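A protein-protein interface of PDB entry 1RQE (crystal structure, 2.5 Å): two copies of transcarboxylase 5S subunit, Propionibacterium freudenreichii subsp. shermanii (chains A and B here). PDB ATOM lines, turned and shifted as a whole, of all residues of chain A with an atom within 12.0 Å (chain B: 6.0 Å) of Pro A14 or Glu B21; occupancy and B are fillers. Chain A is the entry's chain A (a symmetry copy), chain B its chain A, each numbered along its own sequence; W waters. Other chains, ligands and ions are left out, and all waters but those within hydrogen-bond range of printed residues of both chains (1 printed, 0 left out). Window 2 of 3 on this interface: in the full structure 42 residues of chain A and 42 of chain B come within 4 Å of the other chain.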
ATOM      1  N   PRO A  14       9.581 -19.142 -20.250  1.00  0.00           N
ATOM      2  CA  PRO A  14      10.090 -18.804 -18.893  1.00  0.00           C
ATOM      3  C   PRO A  14       9.142 -19.303 -17.796  1.00  0.00           C
ATOM      4  O   PRO A  14       8.557 -18.505 -17.055  1.00  0.00           O
ATOM      5  CB  PRO A  14      10.228 -17.284 -18.831  1.00  0.00           C
ATOM      6  CG  PRO A  14      10.356 -16.920 -20.323  1.00  0.00           C
ATOM      7  CD  PRO A  14       9.429 -17.913 -21.053  1.00  0.00           C
ATOM      8  N   ARG A  15       8.997 -20.622 -17.698  1.00  0.00           N
ATOM      9  CA  ARG A  15       8.119 -21.228 -16.702  1.00  0.00           C
ATOM     10  C   ARG A  15       8.612 -20.938 -15.270  1.00  0.00           C
ATOM     11  O   ARG A  15       9.798 -21.080 -14.975  1.00  0.00           O
ATOM     12  CB  ARG A  15       8.060 -22.726 -16.959  1.00  0.00           C
ATOM     13  CG  ARG A  15       6.842 -23.418 -16.399  1.00  0.00           C
ATOM     14  CD  ARG A  15       7.017 -24.918 -16.542  1.00  0.00           C
ATOM     15  NE  ARG A  15       5.939 -25.678 -15.924  1.00  0.00           N
ATOM     16  CZ  ARG A  15       6.106 -26.857 -15.334  1.00  0.00           C
ATOM     17  NH1 ARG A  15       7.310 -27.414 -15.276  1.00  0.00           N
ATOM     18  NH2 ARG A  15       5.066 -27.478 -14.800  1.00  0.00           N
ATOM     19  N   GLU A  16       7.704 -20.536 -14.382  1.00  0.00           N
ATOM     20  CA  GLU A  16       8.088 -20.204 -13.012  1.00  0.00           C
ATOM     21  C   GLU A  16       7.131 -20.576 -11.904  1.00  0.00           C
ATOM     22  O   GLU A  16       5.923 -20.625 -12.101  1.00  0.00           O
ATOM     23  CB  GLU A  16       8.364 -18.713 -12.911  1.00  0.00           C
ATOM     24  CG  GLU A  16       9.566 -18.298 -13.716  1.00  0.00           C
ATOM     25  CD  GLU A  16       9.882 -16.838 -13.583  1.00  0.00           C
ATOM     26  OE1 GLU A  16      11.042 -16.473 -13.874  1.00  0.00           O
ATOM     27  OE2 GLU A  16       8.973 -16.066 -13.198  1.00  0.00           O
ATOM     28  N   ILE A  17       7.689 -20.828 -10.724  1.00  0.00           N
ATOM     29  CA  ILE A  17       6.900 -21.162  -9.550  1.00  0.00           C
ATOM     30  C   ILE A  17       7.134 -20.104  -8.473  1.00  0.00           C
ATOM     31  O   ILE A  17       8.271 -19.735  -8.183  1.00  0.00           O
ATOM     32  CB  ILE A  17       7.280 -22.539  -8.983  1.00  0.00           C
ATOM     33  CG1 ILE A  17       7.001 -23.618 -10.021  1.00  0.00           C
ATOM     34  CG2 ILE A  17       6.444 -22.846  -7.734  1.00  0.00           C
ATOM     35  CD1 ILE A  17       7.376 -24.990  -9.555  1.00  0.00           C
ATOM     36  N   GLU A  18       6.058 -19.598  -7.886  1.00  0.00           N
ATOM     37  CA  GLU A  18       6.186 -18.593  -6.847  1.00  0.00           C
ATOM     38  C   GLU A  18       6.414 -19.283  -5.509  1.00  0.00           C
ATOM     39  O   GLU A  18       5.677 -20.196  -5.143  1.00  0.00           O
ATOM     40  CB  GLU A  18       4.922 -17.734  -6.801  1.00  0.00           C
ATOM     41  CG  GLU A  18       4.823 -16.825  -5.594  1.00  0.00           C
ATOM     42  CD  GLU A  18       3.893 -15.652  -5.824  1.00  0.00           C
ATOM     43  OE1 GLU A  18       4.301 -14.706  -6.533  1.00  0.00           O
ATOM     44  OE2 GLU A  18       2.756 -15.677  -5.305  1.00  0.00           O
ATOM     45  N   GLN A 204       2.658 -31.629  -5.464  1.00  0.00           N
ATOM     46  CA  GLN A 204       1.852 -30.567  -6.059  1.00  0.00           C
ATOM     47  C   GLN A 204       0.650 -30.237  -5.169  1.00  0.00           C
ATOM     48  O   GLN A 204       0.431 -29.081  -4.806  1.00  0.00           O
ATOM     49  CB  GLN A 204       1.386 -30.961  -7.462  1.00  0.00           C
ATOM     50  CG  GLN A 204       0.891 -29.775  -8.275  1.00  0.00           C
ATOM     51  CD  GLN A 204       1.944 -28.686  -8.391  1.00  0.00           C
ATOM     52  OE1 GLN A 204       3.011 -28.901  -8.970  1.00  0.00           O
ATOM     53  NE2 GLN A 204       1.654 -27.515  -7.835  1.00  0.00           N
ATOM     54  N   GLU B  18      12.618 -20.465 -11.370  1.00  0.00           N
ATOM     55  CA  GLU B  18      12.392 -20.890 -12.739  1.00  0.00           C
ATOM     56  C   GLU B  18      12.538 -22.403 -12.824  1.00  0.00           C
ATOM     57  O   GLU B  18      13.525 -22.963 -12.352  1.00  0.00           O
ATOM     58  CB  GLU B  18      13.391 -20.200 -13.666  1.00  0.00           C
ATOM     59  CG  GLU B  18      13.430 -20.755 -15.075  1.00  0.00           C
ATOM     60  CD  GLU B  18      13.993 -19.767 -16.075  1.00  0.00           C
ATOM     61  OE1 GLU B  18      13.263 -18.819 -16.443  1.00  0.00           O
ATOM     62  OE2 GLU B  18      15.162 -19.929 -16.487  1.00  0.00           O
ATOM     63  N   VAL B  19      11.553 -23.072 -13.408  1.00  0.00           N
ATOM     64  CA  VAL B  19      11.623 -24.517 -13.534  1.00  0.00           C
ATOM     65  C   VAL B  19      11.536 -24.944 -14.992  1.00  0.00           C
ATOM     66  O   VAL B  19      10.929 -24.254 -15.811  1.00  0.00           O
ATOM     67  CB  VAL B  19      10.506 -25.193 -12.735  1.00  0.00           C
ATOM     68  CG1 VAL B  19      10.647 -24.818 -11.280  1.00  0.00           C
ATOM     69  CG2 VAL B  19       9.149 -24.774 -13.272  1.00  0.00           C
ATOM     70  N   SER B  20      12.146 -26.082 -15.310  1.00  0.00           N
ATOM     71  CA  SER B  20      12.151 -26.579 -16.678  1.00  0.00           C
ATOM     72  C   SER B  20      10.736 -26.807 -17.213  1.00  0.00           C
ATOM     73  O   SER B  20       9.783 -27.002 -16.450  1.00  0.00           O
ATOM     74  CB  SER B  20      12.976 -27.871 -16.768  1.00  0.00           C
ATOM     75  OG  SER B  20      12.427 -28.908 -15.974  1.00  0.00           O
ATOM     76  N   GLU B  21      10.602 -26.759 -18.534  1.00  0.00           N
ATOM     77  CA  GLU B  21       9.307 -26.960 -19.179  1.00  0.00           C
ATOM     78  C   GLU B  21       8.794 -28.375 -18.921  1.00  0.00           C
ATOM     79  O   GLU B  21       9.574 -29.316 -18.787  1.00  0.00           O
ATOM     80  CB  GLU B  21       9.423 -26.700 -20.691  1.00  0.00           C
ATOM     81  CG  GLU B  21       8.760 -25.379 -21.168  1.00  0.00           C
ATOM     82  CD  GLU B  21       9.415 -24.097 -20.621  1.00  0.00           C
ATOM     83  OE1 GLU B  21       8.854 -23.000 -20.849  1.00  0.00           O
ATOM     84  OE2 GLU B  21      10.487 -24.175 -19.974  1.00  0.00           O
ATOM     85  N   PRO B  22       7.469 -28.537 -18.828  1.00  0.00           N
ATOM     86  CA  PRO B  22       6.850 -29.847 -18.583  1.00  0.00           C
ATOM     87  C   PRO B  22       7.487 -30.863 -19.496  1.00  0.00           C
ATOM     88  O   PRO B  22       7.697 -30.574 -20.669  1.00  0.00           O
ATOM     89  CB  PRO B  22       5.392 -29.605 -18.922  1.00  0.00           C
ATOM     90  CG  PRO B  22       5.205 -28.187 -18.471  1.00  0.00           C
ATOM     91  CD  PRO B  22       6.444 -27.496 -19.004  1.00  0.00           C
ATOM     92  N   ARG B  23       7.809 -32.042 -18.971  1.00  0.00           N
ATOM     93  CA  ARG B  23       8.456 -33.049 -19.797  1.00  0.00           C
ATOM     94  C   ARG B  23       8.558 -34.401 -19.108  1.00  0.00           C
ATOM     95  O   ARG B  23       8.326 -34.536 -17.897  1.00  0.00           O
ATOM     96  CB  ARG B  23       9.864 -32.583 -20.177  1.00  0.00           C
ATOM     97  CG  ARG B  23      10.854 -32.691 -19.039  1.00  0.00           C
ATOM     98  CD  ARG B  23      11.583 -31.381 -18.779  1.00  0.00           C
ATOM     99  NE  ARG B  23      12.315 -31.428 -17.510  1.00  0.00           N
ATOM    100  CZ  ARG B  23      13.306 -32.275 -17.252  1.00  0.00           C
ATOM    101  NH1 ARG B  23      13.688 -33.139 -18.178  1.00  0.00           N
ATOM    102  NH2 ARG B  23      13.901 -32.276 -16.062  1.00  0.00           N
ATOM    103  N   GLY B 276       3.669 -31.505 -13.883  1.00  0.00           N
ATOM    104  CA  GLY B 276       3.939 -31.189 -15.269  1.00  0.00           C
ATOM    105  C   GLY B 276       4.976 -32.187 -15.738  1.00  0.00           C
ATOM    106  O   GLY B 276       5.095 -32.473 -16.931  1.00  0.00           O
ATOM    107  N   TYR B 277       5.736 -32.721 -14.789  1.00  0.00           N
ATOM    108  CA  TYR B 277       6.743 -33.724 -15.111  1.00  0.00           C
ATOM    109  C   TYR B 277       6.113 -35.097 -14.936  1.00  0.00           C
ATOM    110  O   TYR B 277       5.167 -35.259 -14.168  1.00  0.00           O
ATOM    111  CB  TYR B 277       7.940 -33.612 -14.181  1.00  0.00           C
ATOM    112  CG  TYR B 277       8.522 -32.236 -14.130  1.00  0.00           C
ATOM    113  CD1 TYR B 277       8.373 -31.450 -12.992  1.00  0.00           C
ATOM    114  CD2 TYR B 277       9.235 -31.716 -15.213  1.00  0.00           C
ATOM    115  CE1 TYR B 277       8.914 -30.185 -12.923  1.00  0.00           C
ATOM    116  CE2 TYR B 277       9.787 -30.447 -15.157  1.00  0.00           C
ATOM    117  CZ  TYR B 277       9.621 -29.687 -14.003  1.00  0.00           C
ATOM    118  OH  TYR B 277      10.141 -28.427 -13.919  1.00  0.00           O
HETATM  119  O   HOH W   1      13.783 -16.709 -13.866  1.00  0.00           O
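N of Pro A14 touches OE1 of Glu B21, at 3.97 Å.
Arg A15 touches Glu B18.
Glu B21 touches Arg A15 (OE1 to N, 3.95 Å).
Arg A15 touches Pro B22 (CZ to CG, 3.5 Å).
CA of Gly B276 touches NH2 of Arg A15, 3.9 Å away.
Glu A16 touches Glu B18 (CG to CA, 3.96 Å).
Val B19 touches Ile A17.
Position printed for both chains: 18.
The backbone NH (N) of Val B19 is in hydrogen-bond range of the backbone carbonyl oxygen (O) of Arg A15, at 3.1 Å.
The backbone carbonyl oxygen (O) of Ser B20 is in hydrogen-bond range of the guanidinium group (NH1) of Arg A15, at 2.8 Å.
The side-chain hydroxyl (OH) of Tyr B277 sits at hydrogen-bond distance from the guanidinium group (NH1) of Arg A15.
Printed residues of chain A that touch a printed residue of chain B: Pro A14, Arg A15, Glu A16 and Ile A17.
Hydrophobic or aromatic side chains of chain A within 4 Å of the printed part of chain B: Ile A17.
Along chain A the printed residues that touch a printed residue of chain B span positions 14 to 17.
Of the 8 printed residues of chain B, 7 touch a printed residue of chain A.
Printed residues of chain B that touch a printed residue of chain A: Glu B18, Val B19, Ser B20, Glu B21, Pro B22, Gly B276 and Tyr B277.
Hydrophobic or aromatic side chains of chain B that line the printed part of chain A: Val B19, Pro B22 and Tyr B277.
Among the printed residues, 10 pairs touch across the chains.
Among the printed residues, no Asp or Glu carboxylate lies within 4 Å of a Lys or Arg side-chain nitrogen of the other chain.
Water W1 lies within hydrogen-bond range of the side-chain carboxylate (OE1) of Glu A16 (2.8 Å) and the side-chain carboxylate (OE1) of Glu B18 (3.4 Å).
OG of Ser B20 lies within hydrogen-bond range of NE of Arg B23 (3.0 Å).
The side-chain hydroxyl of Tyr B277 lies within hydrogen-bond range of the backbone carbonyl oxygen of Ser B20.
The backbone NH (N) of Arg B23 lies within hydrogen-bond range of the backbone carbonyl oxygen (O) of Gly B276, 3.4 Å away.
Printed residues of chain B within 4 Å of Pro A14: Glu B21 (3.97 Å).
Printed residues of chain B within 4 Å of Arg A15: Glu B18 (3.4 Å), Val B19 (3.1 Å), Ser B20 (2.8 Å), Glu B21 (3.95 Å), Pro B22 (3.5 Å), Gly B276 (3.9 Å) and Tyr B277 (3.3 Å).
Printed residues of chain B within 4 Å of Glu A16: Glu B18 (3.96 Å).
Of the printed residues of chain B, Ile A17 touches Val B19 (3.7 Å).
Val B19 touches just these residues of chain A: Arg A15 (3.1 Å) and Ile A17 (3.7 Å).
Pro B22 touches one residue of chain A.
No residue of chain A comes within 4 Å of Arg B23.
Of chain A, only Arg A15 comes within 4 Å of Gly B276.
Printed residues of chain A within 4 Å of Tyr B277: Arg A15 (3.3 Å).
The nearest residue of chain A that does not touch Glu B21 is Glu A16 (7.0 Å).
The nearest printed residue of chain B that does not touch Ile A17 is Glu B18 (5.0 Å).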
